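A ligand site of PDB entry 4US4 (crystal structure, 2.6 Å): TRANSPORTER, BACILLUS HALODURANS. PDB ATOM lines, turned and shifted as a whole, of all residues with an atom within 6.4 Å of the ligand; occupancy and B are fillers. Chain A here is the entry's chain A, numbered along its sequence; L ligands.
A nitrogen (N1) of the ligand is in hydrogen-bond range of the backbone carbonyl oxygen of Phe 232, at 2.7 Å.
O1 of the ligand is in hydrogen-bond range of N of Gly 32.
The backbone NH (N) of Ser 235 sits close to a nitrogen (N1) of the ligand (3.5 Å).
OG of Ser 235 sits at hydrogen-bond distance from N1 of the ligand.
The backbone carbonyl oxygen (O) of Ala 28 sits at hydrogen-bond distance from a nitrogen (N1) of the ligand, at 3.0 Å.
The backbone NH (N) of Leu 31 lies within hydrogen-bond range of an oxygen (O1) of the ligand (3.0 Å).
An oxygen (O1) of the ligand sits at hydrogen-bond distance from the side-chain hydroxyl (OH) of Tyr 110, 3.1 Å away.
The backbone carbonyl oxygen (O) of Thr 233 lies within hydrogen-bond range of a nitrogen (N1) of the ligand (3.2 Å).
OD1 of Asn 33 lies close to O2 of the ligand, 3.5 Å away.
O of Gly 32 sits at hydrogen-bond distance from NE2 of Gln 229, 2.9 Å away.
The side-chain hydroxyl (OH) of Tyr 110 sits at hydrogen-bond distance from the backbone NH (N) of Leu 31 (2.9 Å).
The side-chain hydroxyl (OG1) of Thr 233 sits at hydrogen-bond distance from the side-chain carboxylate (OD2) of Asp 265.
The backbone NH (N) of Gly 30 sits at hydrogen-bond distance from the side-chain amide oxygen (OD1) of Asn 33 (2.6 Å).
The side-chain hydroxyl of Ser 326 is in hydrogen-bond range of the backbone carbonyl oxygen of Ser 27 (2.9 Å).
O of Asp 265 sits at hydrogen-bond distance from ND2 of Asn 33 (3.1 Å).
The side-chain hydroxyl (OG) of Ser 326 is in hydrogen-bond range of the backbone carbonyl oxygen (O) of Ala 322 (3.1 Å).
The backbone NH (N) of Leu 236 is in hydrogen-bond range of the backbone carbonyl oxygen (O) of Phe 231 (2.9 Å).
Ser 27 touches the ligand (O to C1, 3.4 Å).
Gly 30 touches the ligand (C to O1, 3.2 Å).
Ile 106 touches the ligand (CD1 to C10, 3.9 Å).
Phe 231 touches the ligand (O to C10, 3.9 Å).
N of Leu 236 touches C11 of the ligand, at 3.9 Å.
Met 238 touches the ligand.
Ala 240 touches the ligand (CB to C9, 3.99 Å).
O of Ser 326 touches C5 of the ligand, at 3.6 Å.
OG of Ser 329 touches N2 of the ligand, at 3.7 Å.
CD2 of Leu 330 touches C7 of the ligand (3.4 Å).
Leu 395 touches the ligand (CD1 to C10, 3.8 Å).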
ATOM      1  N   SER A  27      23.649  -4.410 -10.694  1.00  0.00           N
ATOM      2  CA  SER A  27      24.032  -5.720 -10.189  1.00  0.00           C
ATOM      3  C   SER A  27      23.419  -6.838 -11.026  1.00  0.00           C
ATOM      4  O   SER A  27      24.105  -7.809 -11.364  1.00  0.00           O
ATOM      5  CB  SER A  27      23.591  -5.865  -8.719  1.00  0.00           C
ATOM      6  OG  SER A  27      23.735  -7.203  -8.287  1.00  0.00           O
ATOM      7  N   ALA A  28      22.138  -6.695 -11.349  1.00  0.00           N
ATOM      8  CA  ALA A  28      21.404  -7.722 -12.067  1.00  0.00           C
ATOM      9  C   ALA A  28      21.945  -7.954 -13.467  1.00  0.00           C
ATOM     10  O   ALA A  28      22.148  -9.093 -13.869  1.00  0.00           O
ATOM     11  CB  ALA A  28      19.926  -7.352 -12.133  1.00  0.00           C
ATOM     12  N   VAL A  29      22.184  -6.869 -14.198  1.00  0.00           N
ATOM     13  CA  VAL A  29      22.661  -6.975 -15.572  1.00  0.00           C
ATOM     14  C   VAL A  29      24.171  -7.176 -15.618  1.00  0.00           C
ATOM     15  O   VAL A  29      24.937  -6.326 -15.167  1.00  0.00           O
ATOM     16  CB  VAL A  29      22.297  -5.710 -16.390  1.00  0.00           C
ATOM     17  CG1 VAL A  29      22.893  -5.802 -17.790  1.00  0.00           C
ATOM     18  CG2 VAL A  29      20.786  -5.543 -16.461  1.00  0.00           C
ATOM     19  N   GLY A  30      24.585  -8.319 -16.161  1.00  0.00           N
ATOM     20  CA  GLY A  30      25.995  -8.646 -16.249  1.00  0.00           C
ATOM     21  C   GLY A  30      26.265  -9.815 -17.173  1.00  0.00           C
ATOM     22  O   GLY A  30      25.584  -9.997 -18.178  1.00  0.00           O
ATOM     23  N   LEU A  31      27.270 -10.614 -16.821  1.00  0.00           N
ATOM     24  CA  LEU A  31      27.696 -11.747 -17.650  1.00  0.00           C
ATOM     25  C   LEU A  31      26.620 -12.829 -17.736  1.00  0.00           C
ATOM     26  O   LEU A  31      26.615 -13.636 -18.667  1.00  0.00           O
ATOM     27  CB  LEU A  31      28.996 -12.344 -17.108  1.00  0.00           C
ATOM     28  CG  LEU A  31      30.164 -11.371 -17.001  1.00  0.00           C
ATOM     29  CD1 LEU A  31      31.425 -12.082 -16.519  1.00  0.00           C
ATOM     30  CD2 LEU A  31      30.417 -10.679 -18.337  1.00  0.00           C
ATOM     31  N   GLY A  32      25.710 -12.842 -16.765  1.00  0.00           N
ATOM     32  CA  GLY A  32      24.632 -13.810 -16.769  1.00  0.00           C
ATOM     33  C   GLY A  32      23.641 -13.559 -17.885  1.00  0.00           C
ATOM     34  O   GLY A  32      22.938 -14.463 -18.325  1.00  0.00           O
ATOM     35  N   ASN A  33      23.599 -12.317 -18.357  1.00  0.00           N
ATOM     36  CA  ASN A  33      22.659 -11.920 -19.402  1.00  0.00           C
ATOM     37  C   ASN A  33      23.143 -12.286 -20.797  1.00  0.00           C
ATOM     38  O   ASN A  33      22.354 -12.659 -21.665  1.00  0.00           O
ATOM     39  CB  ASN A  33      22.400 -10.415 -19.340  1.00  0.00           C
ATOM     40  CG  ASN A  33      21.909  -9.970 -17.991  1.00  0.00           C
ATOM     41  OD1 ASN A  33      22.678  -9.924 -17.027  1.00  0.00           O
ATOM     42  ND2 ASN A  33      20.629  -9.614 -17.913  1.00  0.00           N
ATOM     43  N   ILE A 106      30.227 -18.240  -6.563  1.00  0.00           N
ATOM     44  CA  ILE A 106      29.862 -17.567  -7.805  1.00  0.00           C
ATOM     45  C   ILE A 106      30.944 -16.593  -8.254  1.00  0.00           C
ATOM     46  O   ILE A 106      31.329 -16.591  -9.431  1.00  0.00           O
ATOM     47  CB  ILE A 106      28.523 -16.808  -7.664  1.00  0.00           C
ATOM     48  CG1 ILE A 106      27.381 -17.801  -7.452  1.00  0.00           C
ATOM     49  CG2 ILE A 106      28.257 -15.960  -8.906  1.00  0.00           C
ATOM     50  CD1 ILE A 106      26.005 -17.171  -7.461  1.00  0.00           C
ATOM     51  N   TYR A 110      33.179 -16.214 -11.618  1.00  0.00           N
ATOM     52  CA  TYR A 110      32.727 -15.003 -12.297  1.00  0.00           C
ATOM     53  C   TYR A 110      33.916 -14.138 -12.693  1.00  0.00           C
ATOM     54  O   TYR A 110      33.926 -13.538 -13.768  1.00  0.00           O
ATOM     55  CB  TYR A 110      31.763 -14.213 -11.402  1.00  0.00           C
ATOM     56  CG  TYR A 110      30.901 -13.209 -12.149  1.00  0.00           C
ATOM     57  CD1 TYR A 110      31.344 -11.905 -12.357  1.00  0.00           C
ATOM     58  CD2 TYR A 110      29.654 -13.573 -12.633  1.00  0.00           C
ATOM     59  CE1 TYR A 110      30.558 -10.987 -13.036  1.00  0.00           C
ATOM     60  CE2 TYR A 110      28.868 -12.655 -13.313  1.00  0.00           C
ATOM     61  CZ  TYR A 110      29.315 -11.366 -13.504  1.00  0.00           C
ATOM     62  OH  TYR A 110      28.537 -10.460 -14.183  1.00  0.00           O
ATOM     63  N   GLN A 229      19.340 -20.233 -13.851  1.00  0.00           N
ATOM     64  CA  GLN A 229      19.595 -19.031 -14.637  1.00  0.00           C
ATOM     65  C   GLN A 229      18.731 -17.871 -14.149  1.00  0.00           C
ATOM     66  O   GLN A 229      19.167 -16.730 -14.140  1.00  0.00           O
ATOM     67  CB  GLN A 229      19.325 -19.308 -16.120  1.00  0.00           C
ATOM     68  CG  GLN A 229      19.520 -18.108 -17.022  1.00  0.00           C
ATOM     69  CD  GLN A 229      20.933 -17.566 -16.974  1.00  0.00           C
ATOM     70  OE1 GLN A 229      21.900 -18.312 -16.828  1.00  0.00           O
ATOM     71  NE2 GLN A 229      21.066 -16.244 -17.090  1.00  0.00           N
ATOM     72  N   PHE A 231      17.617 -17.279 -11.039  1.00  0.00           N
ATOM     73  CA  PHE A 231      18.161 -16.734  -9.800  1.00  0.00           C
ATOM     74  C   PHE A 231      19.499 -16.045 -10.042  1.00  0.00           C
ATOM     75  O   PHE A 231      19.828 -15.057  -9.385  1.00  0.00           O
ATOM     76  CB  PHE A 231      18.328 -17.840  -8.756  1.00  0.00           C
ATOM     77  CG  PHE A 231      17.073 -18.118  -7.972  1.00  0.00           C
ATOM     78  CD1 PHE A 231      16.778 -17.396  -6.830  1.00  0.00           C
ATOM     79  CD2 PHE A 231      16.192 -19.113  -8.369  1.00  0.00           C
ATOM     80  CE1 PHE A 231      15.633 -17.649  -6.102  1.00  0.00           C
ATOM     81  CE2 PHE A 231      15.047 -19.374  -7.648  1.00  0.00           C
ATOM     82  CZ  PHE A 231      14.760 -18.647  -6.510  1.00  0.00           C
ATOM     83  N   PHE A 232      20.269 -16.564 -10.994  1.00  0.00           N
ATOM     84  CA  PHE A 232      21.584 -16.021 -11.303  1.00  0.00           C
ATOM     85  C   PHE A 232      21.491 -14.641 -11.957  1.00  0.00           C
ATOM     86  O   PHE A 232      22.190 -13.716 -11.575  1.00  0.00           O
ATOM     87  CB  PHE A 232      22.366 -16.987 -12.213  1.00  0.00           C
ATOM     88  CG  PHE A 232      23.823 -16.631 -12.372  1.00  0.00           C
ATOM     89  CD1 PHE A 232      24.230 -15.708 -13.316  1.00  0.00           C
ATOM     90  CD2 PHE A 232      24.774 -17.251 -11.591  1.00  0.00           C
ATOM     91  CE1 PHE A 232      25.571 -15.390 -13.469  1.00  0.00           C
ATOM     92  CE2 PHE A 232      26.122 -16.937 -11.737  1.00  0.00           C
ATOM     93  CZ  PHE A 232      26.513 -16.007 -12.677  1.00  0.00           C
ATOM     94  N   THR A 233      20.619 -14.527 -12.957  1.00  0.00           N
ATOM     95  CA  THR A 233      20.528 -13.302 -13.739  1.00  0.00           C
ATOM     96  C   THR A 233      19.904 -12.157 -12.930  1.00  0.00           C
ATOM     97  O   THR A 233      20.165 -10.987 -13.201  1.00  0.00           O
ATOM     98  CB  THR A 233      19.732 -13.528 -15.040  1.00  0.00           C
ATOM     99  OG1 THR A 233      19.888 -12.409 -15.916  1.00  0.00           O
ATOM    100  CG2 THR A 233      18.252 -13.757 -14.753  1.00  0.00           C
ATOM    101  N   LEU A 234      19.089 -12.501 -11.945  1.00  0.00           N
ATOM    102  CA  LEU A 234      18.379 -11.490 -11.165  1.00  0.00           C
ATOM    103  C   LEU A 234      19.119 -11.108  -9.886  1.00  0.00           C
ATOM    104  O   LEU A 234      18.591 -10.359  -9.063  1.00  0.00           O
ATOM    105  CB  LEU A 234      16.970 -11.975 -10.818  1.00  0.00           C
ATOM    106  CG  LEU A 234      16.002 -12.148 -11.994  1.00  0.00           C
ATOM    107  CD1 LEU A 234      14.628 -12.596 -11.513  1.00  0.00           C
ATOM    108  CD2 LEU A 234      15.899 -10.856 -12.795  1.00  0.00           C
ATOM    109  N   SER A 235      20.341 -11.617  -9.737  1.00  0.00           N
ATOM    110  CA  SER A 235      21.130 -11.412  -8.522  1.00  0.00           C
ATOM    111  C   SER A 235      20.326 -11.825  -7.301  1.00  0.00           C
ATOM    112  O   SER A 235      20.311 -11.122  -6.285  1.00  0.00           O
ATOM    113  CB  SER A 235      21.586  -9.953  -8.399  1.00  0.00           C
ATOM    114  OG  SER A 235      22.373  -9.575  -9.521  1.00  0.00           O
ATOM    115  N   LEU A 236      19.661 -12.964  -7.401  1.00  0.00           N
ATOM    116  CA  LEU A 236      18.662 -13.370  -6.423  1.00  0.00           C
ATOM    117  C   LEU A 236      19.064 -14.653  -5.701  1.00  0.00           C
ATOM    118  O   LEU A 236      19.696 -15.531  -6.279  1.00  0.00           O
ATOM    119  CB  LEU A 236      17.312 -13.563  -7.124  1.00  0.00           C
ATOM    120  CG  LEU A 236      16.050 -13.706  -6.268  1.00  0.00           C
ATOM    121  CD1 LEU A 236      15.777 -12.422  -5.508  1.00  0.00           C
ATOM    122  CD2 LEU A 236      14.870 -14.077  -7.148  1.00  0.00           C
ATOM    123  N   GLY A 237      18.685 -14.751  -4.427  1.00  0.00           N
ATOM    124  CA  GLY A 237      18.874 -15.974  -3.674  1.00  0.00           C
ATOM    125  C   GLY A 237      19.999 -15.936  -2.651  1.00  0.00           C
ATOM    126  O   GLY A 237      20.073 -16.815  -1.793  1.00  0.00           O
ATOM    127  N   MET A 238      20.869 -14.936  -2.738  1.00  0.00           N
ATOM    128  CA  MET A 238      21.995 -14.855  -1.810  1.00  0.00           C
ATOM    129  C   MET A 238      21.905 -13.634  -0.898  1.00  0.00           C
ATOM    130  O   MET A 238      22.709 -13.493   0.024  1.00  0.00           O
ATOM    131  CB  MET A 238      23.321 -14.839  -2.570  1.00  0.00           C
ATOM    132  CG  MET A 238      23.659 -13.513  -3.222  1.00  0.00           C
ATOM    133  SD  MET A 238      25.415 -13.397  -3.604  1.00  0.00           S
ATOM    134  CE  MET A 238      25.696 -14.965  -4.434  1.00  0.00           C
ATOM    135  N   GLY A 239      20.934 -12.766  -1.155  1.00  0.00           N
ATOM    136  CA  GLY A 239      20.728 -11.607  -0.315  1.00  0.00           C
ATOM    137  C   GLY A 239      21.483 -10.377  -0.797  1.00  0.00           C
ATOM    138  O   GLY A 239      21.804  -9.493  -0.005  1.00  0.00           O
ATOM    139  N   ALA A 240      21.766 -10.328  -2.092  1.00  0.00           N
ATOM    140  CA  ALA A 240      22.396  -9.156  -2.683  1.00  0.00           C
ATOM    141  C   ALA A 240      21.388  -8.021  -2.823  1.00  0.00           C
ATOM    142  O   ALA A 240      21.725  -6.851  -2.651  1.00  0.00           O
ATOM    143  CB  ALA A 240      23.007  -9.495  -4.025  1.00  0.00           C
ATOM    144  N   ASP A 265      16.352  -6.697 -17.047  1.00  0.00           N
ATOM    145  CA  ASP A 265      17.313  -7.785 -17.093  1.00  0.00           C
ATOM    146  C   ASP A 265      16.890  -8.861 -18.081  1.00  0.00           C
ATOM    147  O   ASP A 265      17.717  -9.413 -18.815  1.00  0.00           O
ATOM    148  CB  ASP A 265      17.508  -8.388 -15.701  1.00  0.00           C
ATOM    149  CG  ASP A 265      18.468  -9.559 -15.697  1.00  0.00           C
ATOM    150  OD1 ASP A 265      19.694  -9.328 -15.754  1.00  0.00           O
ATOM    151  OD2 ASP A 265      17.985 -10.713 -15.638  1.00  0.00           O
ATOM    152  N   ALA A 322      29.788  -3.784 -17.103  1.00  0.00           N
ATOM    153  CA  ALA A 322      28.637  -4.502 -16.562  1.00  0.00           C
ATOM    154  C   ALA A 322      29.083  -5.627 -15.644  1.00  0.00           C
ATOM    155  O   ALA A 322      28.481  -5.876 -14.606  1.00  0.00           O
ATOM    156  CB  ALA A 322      27.764  -5.040 -17.685  1.00  0.00           C
ATOM    157  N   SER A 325      30.504  -4.136 -12.276  1.00  0.00           N
ATOM    158  CA  SER A 325      29.450  -3.682 -11.379  1.00  0.00           C
ATOM    159  C   SER A 325      28.681  -4.848 -10.775  1.00  0.00           C
ATOM    160  O   SER A 325      28.005  -4.695  -9.753  1.00  0.00           O
ATOM    161  CB  SER A 325      28.490  -2.746 -12.127  1.00  0.00           C
ATOM    162  OG  SER A 325      27.886  -3.402 -13.218  1.00  0.00           O
ATOM    163  N   SER A 326      28.787  -6.019 -11.403  1.00  0.00           N
ATOM    164  CA  SER A 326      28.142  -7.216 -10.894  1.00  0.00           C
ATOM    165  C   SER A 326      29.060  -7.941  -9.906  1.00  0.00           C
ATOM    166  O   SER A 326      28.588  -8.548  -8.938  1.00  0.00           O
ATOM    167  CB  SER A 326      27.745  -8.152 -12.040  1.00  0.00           C
ATOM    168  OG  SER A 326      26.642  -7.641 -12.769  1.00  0.00           O
ATOM    169  N   ALA A 327      30.362  -7.868 -10.151  1.00  0.00           N
ATOM    170  CA  ALA A 327      31.345  -8.519  -9.297  1.00  0.00           C
ATOM    171  C   ALA A 327      31.498  -7.782  -7.967  1.00  0.00           C
ATOM    172  O   ALA A 327      31.725  -8.404  -6.931  1.00  0.00           O
ATOM    173  CB  ALA A 327      32.684  -8.620  -9.997  1.00  0.00           C
ATOM    174  N   SER A 329      29.025  -6.199  -6.602  1.00  0.00           N
ATOM    175  CA  SER A 329      27.801  -6.640  -5.948  1.00  0.00           C
ATOM    176  C   SER A 329      27.991  -7.993  -5.275  1.00  0.00           C
ATOM    177  O   SER A 329      27.460  -8.240  -4.196  1.00  0.00           O
ATOM    178  CB  SER A 329      26.659  -6.697  -6.953  1.00  0.00           C
ATOM    179  OG  SER A 329      25.491  -7.244  -6.366  1.00  0.00           O
ATOM    180  N   LEU A 330      28.745  -8.871  -5.939  1.00  0.00           N
ATOM    181  CA  LEU A 330      28.997 -10.211  -5.424  1.00  0.00           C
ATOM    182  C   LEU A 330      29.932 -10.182  -4.210  1.00  0.00           C
ATOM    183  O   LEU A 330      29.646 -10.801  -3.195  1.00  0.00           O
ATOM    184  CB  LEU A 330      29.595 -11.097  -6.521  1.00  0.00           C
ATOM    185  CG  LEU A 330      28.590 -11.708  -7.492  1.00  0.00           C
ATOM    186  CD1 LEU A 330      29.308 -12.323  -8.681  1.00  0.00           C
ATOM    187  CD2 LEU A 330      27.730 -12.739  -6.783  1.00  0.00           C
ATOM    188  N   VAL A 333      28.627  -9.023  -0.558  1.00  0.00           N
ATOM    189  CA  VAL A 333      27.857  -9.909   0.323  1.00  0.00           C
ATOM    190  C   VAL A 333      28.733 -10.602   1.389  1.00  0.00           C
ATOM    191  O   VAL A 333      28.395 -10.550   2.575  1.00  0.00           O
ATOM    192  CB  VAL A 333      27.083 -10.977  -0.494  1.00  0.00           C
ATOM    193  CG1 VAL A 333      26.526 -12.057   0.419  1.00  0.00           C
ATOM    194  CG2 VAL A 333      25.970 -10.323  -1.298  1.00  0.00           C
ATOM    195  N   LEU A 395      21.290 -20.871  -4.503  1.00  0.00           N
ATOM    196  CA  LEU A 395      20.420 -19.758  -4.869  1.00  0.00           C
ATOM    197  C   LEU A 395      18.917 -20.091  -4.822  1.00  0.00           C
ATOM    198  O   LEU A 395      18.149 -19.337  -4.233  1.00  0.00           O
ATOM    199  CB  LEU A 395      20.780 -19.232  -6.271  1.00  0.00           C
ATOM    200  CG  LEU A 395      22.119 -18.502  -6.438  1.00  0.00           C
ATOM    201  CD1 LEU A 395      22.184 -17.840  -7.803  1.00  0.00           C
ATOM    202  CD2 LEU A 395      22.334 -17.486  -5.325  1.00  0.00           C
HETATM  203  N1  LIG L   1      23.048 -11.134 -11.874  1.00  0.00           N
HETATM  204  C1  LIG L   1      24.430 -11.020 -12.336  1.00  0.00           C
HETATM  205  C2  LIG L   1      24.558 -11.478 -13.784  1.00  0.00           C
HETATM  206  O1  LIG L   1      25.621 -11.367 -14.394  1.00  0.00           O
HETATM  207  C3  LIG L   1      25.372 -11.820 -11.441  1.00  0.00           C
HETATM  208  C4  LIG L   1      25.179 -11.559  -9.979  1.00  0.00           C
HETATM  209  C5  LIG L   1      25.551 -10.445  -9.289  1.00  0.00           C
HETATM  210  C6  LIG L   1      24.549 -12.428  -9.031  1.00  0.00           C
HETATM  211  N2  LIG L   1      25.198 -10.561  -7.960  1.00  0.00           N
HETATM  212  C7  LIG L   1      24.573 -11.777  -7.779  1.00  0.00           C
HETATM  213  C8  LIG L   1      23.954 -13.689  -9.115  1.00  0.00           C
HETATM  214  C9  LIG L   1      24.033 -12.344  -6.624  1.00  0.00           C
HETATM  215  C10 LIG L   1      23.424 -14.259  -7.971  1.00  0.00           C
HETATM  216  C11 LIG L   1      23.467 -13.580  -6.747  1.00  0.00           C
HETATM  217  O2  LIG L   1      23.595 -11.958 -14.374  1.00  0.00           O
